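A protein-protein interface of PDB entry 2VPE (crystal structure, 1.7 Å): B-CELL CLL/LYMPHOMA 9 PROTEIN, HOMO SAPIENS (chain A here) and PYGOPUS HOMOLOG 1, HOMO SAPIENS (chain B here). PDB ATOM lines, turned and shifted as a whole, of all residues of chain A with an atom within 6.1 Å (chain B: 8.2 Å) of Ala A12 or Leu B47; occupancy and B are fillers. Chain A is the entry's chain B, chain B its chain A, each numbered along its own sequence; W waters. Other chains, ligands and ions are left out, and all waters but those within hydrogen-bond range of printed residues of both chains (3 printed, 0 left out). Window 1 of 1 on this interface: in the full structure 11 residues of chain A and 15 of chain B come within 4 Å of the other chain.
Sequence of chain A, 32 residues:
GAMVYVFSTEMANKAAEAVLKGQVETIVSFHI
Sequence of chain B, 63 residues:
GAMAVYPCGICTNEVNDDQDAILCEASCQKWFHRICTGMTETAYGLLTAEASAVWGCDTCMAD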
ATOM      1  N   PHE A   7       5.313  -6.922  20.121  1.00  0.00           N
ATOM      2  CA  PHE A   7       4.227  -7.628  19.419  1.00  0.00           C
ATOM      3  C   PHE A   7       2.857  -7.325  20.009  1.00  0.00           C
ATOM      4  O   PHE A   7       2.677  -7.376  21.221  1.00  0.00           O
ATOM      5  CB  PHE A   7       4.417  -9.137  19.572  1.00  0.00           C
ATOM      6  CG  PHE A   7       5.547  -9.712  18.771  1.00  0.00           C
ATOM      7  CD1 PHE A   7       5.282 -10.419  17.597  1.00  0.00           C
ATOM      8  CD2 PHE A   7       6.872  -9.582  19.198  1.00  0.00           C
ATOM      9  CE1 PHE A   7       6.322 -10.962  16.857  1.00  0.00           C
ATOM     10  CE2 PHE A   7       7.929 -10.140  18.461  1.00  0.00           C
ATOM     11  CZ  PHE A   7       7.658 -10.826  17.293  1.00  0.00           C
ATOM     12  N   SER A   8       1.898  -7.031  19.145  1.00  0.00           N
ATOM     13  CA  SER A   8       0.499  -7.124  19.509  1.00  0.00           C
ATOM     14  C   SER A   8       0.065  -8.587  19.467  1.00  0.00           C
ATOM     15  O   SER A   8       0.799  -9.451  18.983  1.00  0.00           O
ATOM     16  CB  SER A   8      -0.387  -6.314  18.566  1.00  0.00           C
ATOM     17  OG  SER A   8      -0.378  -6.882  17.250  1.00  0.00           O
ATOM     18  N   THR A   9      -1.124  -8.852  19.988  1.00  0.00           N
ATOM     19  CA  THR A   9      -1.687 -10.205  19.926  1.00  0.00           C
ATOM     20  C   THR A   9      -1.855 -10.621  18.463  1.00  0.00           C
ATOM     21  O   THR A   9      -1.467 -11.722  18.076  1.00  0.00           O
ATOM     22  CB  THR A   9      -3.029 -10.298  20.647  1.00  0.00           C
ATOM     23  OG1 THR A   9      -2.820 -10.013  22.039  1.00  0.00           O
ATOM     24  CG2 THR A   9      -3.589 -11.718  20.508  1.00  0.00           C
ATOM     25  N   GLU A  10      -2.393  -9.712  17.663  1.00  0.00           N
ATOM     26  CA  GLU A  10      -2.605  -9.971  16.231  1.00  0.00           C
ATOM     27  C   GLU A  10      -1.289 -10.331  15.549  1.00  0.00           C
ATOM     28  O   GLU A  10      -1.200 -11.320  14.826  1.00  0.00           O
ATOM     29  CB  GLU A  10      -3.243  -8.748  15.553  1.00  0.00           C
ATOM     30  CG  GLU A  10      -3.360  -8.910  14.019  1.00  0.00           C
ATOM     31  CD  GLU A  10      -3.643  -7.592  13.304  1.00  0.00           C
ATOM     32  OE1 GLU A  10      -3.104  -6.548  13.737  1.00  0.00           O
ATOM     33  OE2 GLU A  10      -4.396  -7.614  12.296  1.00  0.00           O
ATOM     34  N   MET A  11      -0.258  -9.536  15.785  1.00  0.00           N
ATOM     35  CA  MET A  11       1.044  -9.808  15.207  1.00  0.00           C
ATOM     36  C   MET A  11       1.664 -11.112  15.696  1.00  0.00           C
ATOM     37  O   MET A  11       2.266 -11.847  14.905  1.00  0.00           O
ATOM     38  CB  MET A  11       2.003  -8.630  15.449  1.00  0.00           C
ATOM     39  CG  MET A  11       1.621  -7.384  14.646  1.00  0.00           C
ATOM     40  SD  MET A  11       1.286  -7.749  12.889  1.00  0.00           S
ATOM     41  CE  MET A  11       2.789  -8.642  12.453  1.00  0.00           C
ATOM     42  N   ALA A  12       1.529 -11.405  16.993  1.00  0.00           N
ATOM     43  CA  ALA A  12       2.069 -12.634  17.558  1.00  0.00           C
ATOM     44  C   ALA A  12       1.376 -13.870  16.960  1.00  0.00           C
ATOM     45  O   ALA A  12       2.025 -14.867  16.656  1.00  0.00           O
ATOM     46  CB  ALA A  12       1.921 -12.634  19.097  1.00  0.00           C
ATOM     47  N   ASN A  13       0.050 -13.798  16.846  1.00  0.00           N
ATOM     48  CA  ASN A  13      -0.734 -14.906  16.271  1.00  0.00           C
ATOM     49  C   ASN A  13      -0.301 -15.161  14.833  1.00  0.00           C
ATOM     50  O   ASN A  13      -0.063 -16.310  14.452  1.00  0.00           O
ATOM     51  CB  ASN A  13      -2.223 -14.615  16.328  1.00  0.00           C
ATOM     52  CG  ASN A  13      -2.821 -14.851  17.715  1.00  0.00           C
ATOM     53  OD1 ASN A  13      -2.172 -15.385  18.621  1.00  0.00           O
ATOM     54  ND2 ASN A  13      -4.065 -14.447  17.877  1.00  0.00           N
ATOM     55  N   LYS A  14      -0.165 -14.081  14.069  1.00  0.00           N
ATOM     56  CA  LYS A  14       0.261 -14.174  12.653  1.00  0.00           C
ATOM     57  C   LYS A  14       1.686 -14.694  12.540  1.00  0.00           C
ATOM     58  O   LYS A  14       1.953 -15.605  11.750  1.00  0.00           O
ATOM     59  CB  LYS A  14       0.150 -12.818  11.958  1.00  0.00           C
ATOM     60  CG  LYS A  14      -1.239 -12.371  11.687  1.00  0.00           C
ATOM     61  CD  LYS A  14      -1.249 -11.234  10.665  1.00  0.00           C
ATOM     62  CE  LYS A  14      -2.674 -10.780  10.367  1.00  0.00           C
ATOM     63  NZ  LYS A  14      -2.656  -9.480   9.607  1.00  0.00           N
ATOM     64  N   ALA A  15       2.606 -14.135  13.339  1.00  0.00           N
ATOM     65  CA  ALA A  15       3.992 -14.599  13.357  1.00  0.00           C
ATOM     66  C   ALA A  15       4.092 -16.085  13.667  1.00  0.00           C
ATOM     67  O   ALA A  15       4.867 -16.809  13.020  1.00  0.00           O
ATOM     68  CB  ALA A  15       4.842 -13.786  14.375  1.00  0.00           C
ATOM     69  N   ALA A  16       3.300 -16.520  14.658  1.00  0.00           N
ATOM     70  CA  ALA A  16       3.295 -17.891  15.145  1.00  0.00           C
ATOM     71  C   ALA A  16       2.918 -18.852  14.007  1.00  0.00           C
ATOM     72  O   ALA A  16       3.557 -19.881  13.825  1.00  0.00           O
ATOM     73  CB  ALA A  16       2.317 -18.027  16.296  1.00  0.00           C
ATOM     74  N   GLU A  17       1.891 -18.497  13.251  1.00  0.00           N
ATOM     75  CA  GLU A  17       1.454 -19.367  12.156  1.00  0.00           C
ATOM     76  C   GLU A  17       2.537 -19.454  11.089  1.00  0.00           C
ATOM     77  O   GLU A  17       2.790 -20.535  10.553  1.00  0.00           O
ATOM     78  CB  GLU A  17       0.097 -18.924  11.599  1.00  0.00           C
ATOM     79  CG  GLU A  17      -1.080 -19.090  12.578  1.00  0.00           C
ATOM     80  CD  GLU A  17      -1.158 -20.502  13.251  1.00  0.00           C
ATOM     81  OE1 GLU A  17      -1.103 -21.522  12.520  1.00  0.00           O
ATOM     82  OE2 GLU A  17      -1.274 -20.592  14.512  1.00  0.00           O
ATOM     83  N   ILE B  22       0.276 -13.610  30.203  1.00  0.00           N
ATOM     84  CA  ILE B  22       1.370 -12.781  29.674  1.00  0.00           C
ATOM     85  C   ILE B  22       1.303 -11.386  30.297  1.00  0.00           C
ATOM     86  O   ILE B  22       0.217 -10.846  30.573  1.00  0.00           O
ATOM     87  CB  ILE B  22       1.374 -12.735  28.114  1.00  0.00           C
ATOM     88  CG1 ILE B  22       2.654 -12.047  27.564  1.00  0.00           C
ATOM     89  CG2 ILE B  22       0.087 -12.161  27.538  1.00  0.00           C
ATOM     90  CD1 ILE B  22       2.946 -12.437  26.124  1.00  0.00           C
ATOM     91  N   LEU B  23       2.476 -10.802  30.488  1.00  0.00           N
ATOM     92  CA  LEU B  23       2.604  -9.468  31.068  1.00  0.00           C
ATOM     93  C   LEU B  23       2.659  -8.437  29.938  1.00  0.00           C
ATOM     94  O   LEU B  23       3.431  -8.623  28.984  1.00  0.00           O
ATOM     95  CB  LEU B  23       3.919  -9.410  31.872  1.00  0.00           C
ATOM     96  CG  LEU B  23       4.201  -8.056  32.518  1.00  0.00           C
ATOM     97  CD1 LEU B  23       3.118  -7.650  33.497  1.00  0.00           C
ATOM     98  CD2 LEU B  23       5.576  -8.155  33.197  1.00  0.00           C
ATOM     99  N   GLU B  25       4.289  -5.913  28.839  1.00  0.00           N
ATOM    100  CA  GLU B  25       5.562  -5.204  29.065  1.00  0.00           C
ATOM    101  C   GLU B  25       5.690  -3.964  28.189  1.00  0.00           C
ATOM    102  O   GLU B  25       6.549  -3.096  28.444  1.00  0.00           O
ATOM    103  CB  GLU B  25       6.739  -6.140  28.845  1.00  0.00           C
ATOM    104  CG  GLU B  25       6.852  -7.238  29.870  1.00  0.00           C
ATOM    105  CD  GLU B  25       7.982  -8.190  29.548  1.00  0.00           C
ATOM    106  OE1 GLU B  25       9.048  -8.080  30.206  1.00  0.00           O
ATOM    107  OE2 GLU B  25       7.823  -9.040  28.630  1.00  0.00           O
ATOM    108  N   THR B  37      -6.913 -12.699  25.988  1.00  0.00           N
ATOM    109  CA  THR B  37      -6.332 -11.864  24.945  1.00  0.00           C
ATOM    110  C   THR B  37      -6.662 -12.356  23.533  1.00  0.00           C
ATOM    111  O   THR B  37      -6.518 -11.607  22.584  1.00  0.00           O
ATOM    112  CB  THR B  37      -4.799 -11.742  25.058  1.00  0.00           C
ATOM    113  OG1 THR B  37      -4.193 -13.000  24.740  1.00  0.00           O
ATOM    114  CG2 THR B  37      -4.357 -11.265  26.459  1.00  0.00           C
ATOM    115  N   GLY B  38      -7.100 -13.604  23.407  1.00  0.00           N
ATOM    116  CA  GLY B  38      -7.307 -14.193  22.076  1.00  0.00           C
ATOM    117  C   GLY B  38      -6.005 -14.688  21.464  1.00  0.00           C
ATOM    118  O   GLY B  38      -5.972 -15.042  20.279  1.00  0.00           O
ATOM    119  N   MET B  39      -4.938 -14.761  22.272  1.00  0.00           N
ATOM    120  CA  MET B  39      -3.649 -15.258  21.806  1.00  0.00           C
ATOM    121  C   MET B  39      -3.643 -16.797  21.719  1.00  0.00           C
ATOM    122  O   MET B  39      -4.124 -17.477  22.634  1.00  0.00           O
ATOM    123  CB  MET B  39      -2.542 -14.778  22.754  1.00  0.00           C
ATOM    124  CG  MET B  39      -1.153 -15.188  22.349  1.00  0.00           C
ATOM    125  SD  MET B  39       0.059 -14.663  23.598  1.00  0.00           S
ATOM    126  CE  MET B  39      -0.064 -12.890  23.402  1.00  0.00           C
ATOM    127  N   THR B  40      -3.144 -17.334  20.607  1.00  0.00           N
ATOM    128  CA  THR B  40      -3.097 -18.796  20.440  1.00  0.00           C
ATOM    129  C   THR B  40      -2.020 -19.406  21.326  1.00  0.00           C
ATOM    130  O   THR B  40      -1.070 -18.725  21.764  1.00  0.00           O
ATOM    131  CB  THR B  40      -2.806 -19.238  18.977  1.00  0.00           C
ATOM    132  OG1 THR B  40      -1.496 -18.801  18.630  1.00  0.00           O
ATOM    133  CG2 THR B  40      -3.838 -18.609  18.011  1.00  0.00           C
ATOM    134  N   GLU B  41      -2.175 -20.690  21.613  1.00  0.00           N
ATOM    135  CA  GLU B  41      -1.140 -21.454  22.307  1.00  0.00           C
ATOM    136  C   GLU B  41       0.217 -21.289  21.612  1.00  0.00           C
ATOM    137  O   GLU B  41       1.263 -21.106  22.264  1.00  0.00           O
ATOM    138  CB  GLU B  41      -1.504 -22.928  22.335  1.00  0.00           C
ATOM    139  CG  GLU B  41      -2.683 -23.213  23.248  1.00  0.00           C
ATOM    140  CD  GLU B  41      -2.909 -24.696  23.436  1.00  0.00           C
ATOM    141  OE1 GLU B  41      -2.107 -25.486  22.916  1.00  0.00           O
ATOM    142  OE2 GLU B  41      -3.896 -25.046  24.109  1.00  0.00           O
ATOM    143  N   THR B  42       0.199 -21.365  20.278  1.00  0.00           N
ATOM    144  CA  THR B  42       1.453 -21.267  19.549  1.00  0.00           C
ATOM    145  C   THR B  42       2.085 -19.871  19.678  1.00  0.00           C
ATOM    146  O   THR B  42       3.299 -19.765  19.863  1.00  0.00           O
ATOM    147  CB  THR B  42       1.280 -21.683  18.078  1.00  0.00           C
ATOM    148  OG1 THR B  42       0.741 -23.006  18.051  1.00  0.00           O
ATOM    149  CG2 THR B  42       2.650 -21.693  17.360  1.00  0.00           C
ATOM    150  N   ALA B  43       1.276 -18.828  19.608  1.00  0.00           N
ATOM    151  CA  ALA B  43       1.785 -17.451  19.764  1.00  0.00           C
ATOM    152  C   ALA B  43       2.366 -17.281  21.172  1.00  0.00           C
ATOM    153  O   ALA B  43       3.433 -16.683  21.355  1.00  0.00           O
ATOM    154  CB  ALA B  43       0.688 -16.456  19.515  1.00  0.00           C
ATOM    155  N   TYR B  44       1.673 -17.851  22.157  1.00  0.00           N
ATOM    156  CA  TYR B  44       2.118 -17.811  23.558  1.00  0.00           C
ATOM    157  C   TYR B  44       3.492 -18.489  23.774  1.00  0.00           C
ATOM    158  O   TYR B  44       4.389 -17.919  24.438  1.00  0.00           O
ATOM    159  CB  TYR B  44       1.029 -18.461  24.418  1.00  0.00           C
ATOM    160  CG  TYR B  44       1.309 -18.465  25.905  1.00  0.00           C
ATOM    161  CD1 TYR B  44       1.148 -17.300  26.651  1.00  0.00           C
ATOM    162  CD2 TYR B  44       1.713 -19.638  26.557  1.00  0.00           C
ATOM    163  CE1 TYR B  44       1.402 -17.305  28.022  1.00  0.00           C
ATOM    164  CE2 TYR B  44       1.952 -19.669  27.921  1.00  0.00           C
ATOM    165  CZ  TYR B  44       1.808 -18.491  28.659  1.00  0.00           C
ATOM    166  OH  TYR B  44       2.032 -18.535  30.020  1.00  0.00           O
ATOM    167  N   GLY B  45       3.674 -19.675  23.180  1.00  0.00           N
ATOM    168  CA  GLY B  45       4.959 -20.401  23.253  1.00  0.00           C
ATOM    169  C   GLY B  45       6.043 -19.620  22.526  1.00  0.00           C
ATOM    170  O   GLY B  45       7.211 -19.572  22.980  1.00  0.00           O
ATOM    171  N   LEU B  46       5.674 -18.992  21.411  1.00  0.00           N
ATOM    172  CA  LEU B  46       6.646 -18.219  20.623  1.00  0.00           C
ATOM    173  C   LEU B  46       7.127 -16.999  21.437  1.00  0.00           C
ATOM    174  O   LEU B  46       8.333 -16.761  21.579  1.00  0.00           O
ATOM    175  CB  LEU B  46       6.053 -17.760  19.290  1.00  0.00           C
ATOM    176  CG  LEU B  46       6.975 -16.866  18.430  1.00  0.00           C
ATOM    177  CD1 LEU B  46       8.224 -17.612  17.965  1.00  0.00           C
ATOM    178  CD2 LEU B  46       6.196 -16.247  17.261  1.00  0.00           C
ATOM    179  N   LEU B  47       6.177 -16.231  21.955  1.00  0.00           N
ATOM    180  CA  LEU B  47       6.524 -15.051  22.761  1.00  0.00           C
ATOM    181  C   LEU B  47       7.339 -15.412  23.986  1.00  0.00           C
ATOM    182  O   LEU B  47       8.266 -14.666  24.341  1.00  0.00           O
ATOM    183  CB  LEU B  47       5.280 -14.241  23.124  1.00  0.00           C
ATOM    184  CG  LEU B  47       4.628 -13.483  21.977  1.00  0.00           C
ATOM    185  CD1 LEU B  47       3.317 -12.907  22.437  1.00  0.00           C
ATOM    186  CD2 LEU B  47       5.563 -12.357  21.468  1.00  0.00           C
ATOM    187  N   THR B  48       7.025 -16.548  24.621  1.00  0.00           N
ATOM    188  CA  THR B  48       7.813 -17.052  25.751  1.00  0.00           C
ATOM    189  C   THR B  48       9.289 -17.267  25.348  1.00  0.00           C
ATOM    190  O   THR B  48      10.203 -16.890  26.085  1.00  0.00           O
ATOM    191  CB  THR B  48       7.211 -18.361  26.339  1.00  0.00           C
ATOM    192  OG1 THR B  48       5.862 -18.106  26.775  1.00  0.00           O
ATOM    193  CG2 THR B  48       8.022 -18.898  27.549  1.00  0.00           C
ATOM    194  N   ALA B  49       9.488 -17.866  24.171  1.00  0.00           N
ATOM    195  CA  ALA B  49      10.823 -18.252  23.662  1.00  0.00           C
ATOM    196  C   ALA B  49      11.648 -17.083  23.117  1.00  0.00           C
ATOM    197  O   ALA B  49      12.874 -17.200  22.972  1.00  0.00           O
ATOM    198  CB  ALA B  49      10.657 -19.302  22.562  1.00  0.00           C
ATOM    199  N   GLU B  50      10.978 -15.991  22.780  1.00  0.00           N
ATOM    200  CA  GLU B  50      11.615 -14.804  22.231  1.00  0.00           C
ATOM    201  C   GLU B  50      12.110 -13.898  23.358  1.00  0.00           C
ATOM    202  O   GLU B  50      11.376 -13.012  23.847  1.00  0.00           O
ATOM    203  CB  GLU B  50      10.641 -14.037  21.351  1.00  0.00           C
ATOM    204  CG  GLU B  50      10.248 -14.759  20.064  1.00  0.00           C
ATOM    205  CD  GLU B  50      11.387 -14.788  19.075  1.00  0.00           C
ATOM    206  OE1 GLU B  50      12.082 -13.750  18.968  1.00  0.00           O
ATOM    207  OE2 GLU B  50      11.594 -15.840  18.433  1.00  0.00           O
ATOM    208  N   ALA B  51      13.362 -14.114  23.739  1.00  0.00           N
ATOM    209  CA  ALA B  51      13.985 -13.325  24.809  1.00  0.00           C
ATOM    210  C   ALA B  51      13.942 -11.819  24.550  1.00  0.00           C
ATOM    211  O   ALA B  51      13.838 -11.039  25.495  1.00  0.00           O
ATOM    212  CB  ALA B  51      15.415 -13.802  25.060  1.00  0.00           C
ATOM    213  N   SER B  52      14.004 -11.400  23.286  1.00  0.00           N
ATOM    214  CA  SER B  52      13.991  -9.973  22.936  1.00  0.00           C
ATOM    215  C   SER B  52      12.612  -9.401  22.622  1.00  0.00           C
ATOM    216  O   SER B  52      12.470  -8.211  22.356  1.00  0.00           O
ATOM    217  CB  SER B  52      14.912  -9.709  21.735  1.00  0.00           C
ATOM    218  OG  SER B  52      16.230 -10.126  22.025  1.00  0.00           O
ATOM    219  N   ALA B  53      11.590 -10.255  22.618  1.00  0.00           N
ATOM    220  CA  ALA B  53      10.245  -9.799  22.317  1.00  0.00           C
ATOM    221  C   ALA B  53       9.486  -9.469  23.593  1.00  0.00           C
ATOM    222  O   ALA B  53       9.696 -10.103  24.620  1.00  0.00           O
ATOM    223  CB  ALA B  53       9.476 -10.855  21.533  1.00  0.00           C
ATOM    224  N   VAL B  54       8.623  -8.473  23.506  1.00  0.00           N
ATOM    225  CA  VAL B  54       7.653  -8.195  24.556  1.00  0.00           C
ATOM    226  C   VAL B  54       6.301  -8.051  23.880  1.00  0.00           C
ATOM    227  O   VAL B  54       6.214  -7.808  22.668  1.00  0.00           O
ATOM    228  CB  VAL B  54       7.949  -6.886  25.358  1.00  0.00           C
ATOM    229  CG1 VAL B  54       9.311  -6.974  26.054  1.00  0.00           C
ATOM    230  CG2 VAL B  54       7.826  -5.663  24.486  1.00  0.00           C
ATOM    231  N   TRP B  55       5.251  -8.201  24.676  1.00  0.00           N
ATOM    232  CA  TRP B  55       3.895  -8.105  24.194  1.00  0.00           C
ATOM    233  C   TRP B  55       3.225  -6.876  24.807  1.00  0.00           C
ATOM    234  O   TRP B  55       3.544  -6.481  25.955  1.00  0.00           O
ATOM    235  CB  TRP B  55       3.133  -9.398  24.564  1.00  0.00           C
ATOM    236  CG  TRP B  55       1.679  -9.364  24.338  1.00  0.00           C
ATOM    237  CD1 TRP B  55       1.022  -9.578  23.151  1.00  0.00           C
ATOM    238  CD2 TRP B  55       0.661  -9.102  25.315  1.00  0.00           C
ATOM    239  NE1 TRP B  55      -0.332  -9.460  23.328  1.00  0.00           N
ATOM    240  CE2 TRP B  55      -0.587  -9.161  24.645  1.00  0.00           C
ATOM    241  CE3 TRP B  55       0.682  -8.782  26.682  1.00  0.00           C
ATOM    242  CZ2 TRP B  55      -1.793  -8.951  25.301  1.00  0.00           C
ATOM    243  CZ3 TRP B  55      -0.534  -8.588  27.341  1.00  0.00           C
ATOM    244  CH2 TRP B  55      -1.745  -8.648  26.648  1.00  0.00           C
ATOM    245  N   GLY B  56       2.344  -6.262  24.018  1.00  0.00           N
ATOM    246  CA  GLY B  56       1.453  -5.202  24.473  1.00  0.00           C
ATOM    247  C   GLY B  56      -0.003  -5.547  24.277  1.00  0.00           C
ATOM    248  O   GLY B  56      -0.367  -6.102  23.233  1.00  0.00           O
HETATM  249  O   HOH W   1      -2.272  -6.632  21.416  1.00  0.00           O
HETATM  250  O   HOH W   2      -5.283  -9.141  22.777  1.00  0.00           O
HETATM  251  O   HOH W   3      -1.176 -18.447  15.947  1.00  0.00           O
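Hydrophobic or aromatic side chains of chain A that line the printed part of chain B: Phe A7, Ala A12 and Ala A16.
Along chain A the printed residues that touch a printed residue of chain B span positions 7 to 16.
Of the 23 printed residues of chain B, 12 touch a printed residue of chain A.
Printed residues of chain B that touch a printed residue of chain A: Thr B37, Gly B38, Met B39, Thr B40, Thr B42, Ala B43, Leu B46, Leu B47, Ala B53, Val B54, Trp B55 and Gly B56.
Among the printed residues, 20 pairs touch across the chains.
Among the printed residues, no Asp or Glu carboxylate lies within 4 Å of a Lys or Arg side-chain nitrogen of the other chain.
Ala A12 touches two residues of chain B.
Leu B47 touches just these residues of chain A: Phe A7 and Ala A12.
Of the printed residues of chain B, Ser A8 touches Trp B55 and Gly B56.
Of the printed residues of chain A, Met B39 touches Thr A9 (3.8 Å) and Asn A13 (3.5 Å).
The nearest residue of chain B that does not touch Ala A12 is Leu B46 (4.4 Å).
The nearest residue of chain A that does not touch Leu B47 is Ser A8 (5.5 Å).
The backbone NH (N) of Phe A7 lies within hydrogen-bond range of the backbone carbonyl oxygen (O) of Val B54, at 2.8 Å.
N of Thr B40 sits at hydrogen-bond distance from OD1 of Asn A13 (2.9 Å).
The backbone NH (N) of Gly B56 is in hydrogen-bond range of the backbone carbonyl oxygen (O) of Phe A7, at 3.0 Å.
ND2 of Asn A13 lies within hydrogen-bond range of O of Gly B38, at 3.1 Å.
The side-chain hydroxyl (OG1) of Thr A9 sits at hydrogen-bond distance from the indole nitrogen (NE1) of Trp B55, at 2.9 Å.
Water W3 lies within hydrogen-bond range of the side-chain carboxylate of Glu A17 (2.6 Å), the side-chain hydroxyl of Thr B40 (2.7 Å) and the backbone carbonyl oxygen of Asn A13 (2.8 Å).
Water W1 lies within hydrogen-bond range of the backbone carbonyl oxygen (O) of Gly B56 (2.7 Å) and the backbone NH (N) of Thr A9 (2.9 Å).
Water W2 bridges the side-chain hydroxyl (OG1) of Thr A9 (2.7 Å) and the backbone carbonyl oxygen (O) of Thr B37 (2.8 Å).
O of Trp B55 is in hydrogen-bond range of N of Glu B25 (3.0 Å).
The side-chain hydroxyl (OG) of Ser A8 lies close to the backbone NH (N) of Glu A10.
The backbone NH (N) of Thr B42 sits close to the side-chain hydroxyl (OG1) of Thr B40 (3.5 Å).
N of Met A11 lies within hydrogen-bond range of OG of Ser A8 (3.0 Å).
The side-chain hydroxyl (OG1) of Thr B37 lies within hydrogen-bond range of the backbone NH (N) of Met B39 (3.1 Å).
The side-chain hydroxyl of Thr B40 sits at hydrogen-bond distance from the backbone NH of Ala B43, 2.9 Å away.
Among the printed residues, merely in contact across the chains: Phe A7 with Leu B47 (3.8 Å), Phe A7 with Ala B53 (3.5 Å), Phe A7 with Trp B55 (3.3 Å), Ser A8 with Trp B55 (3.9 Å), Ser A8 with Gly B56 (3.96 Å), Thr A9 with Thr B37 (3.6 Å), Thr A9 with Gly B38 (3.9 Å), Thr A9 with Met B39 (3.8 Å), Ala A12 with Ala B43 (3.5 Å), Ala A12 with Leu B47 (3.6 Å), Asn A13 with Met B39 (3.5 Å), Asn A13 with Ala B43 (3.2 Å), Ala A16 with Thr B42 (3.8 Å), Ala A16 with Ala B43 (3.6 Å) and Ala A16 with Leu B46 (3.9 Å).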
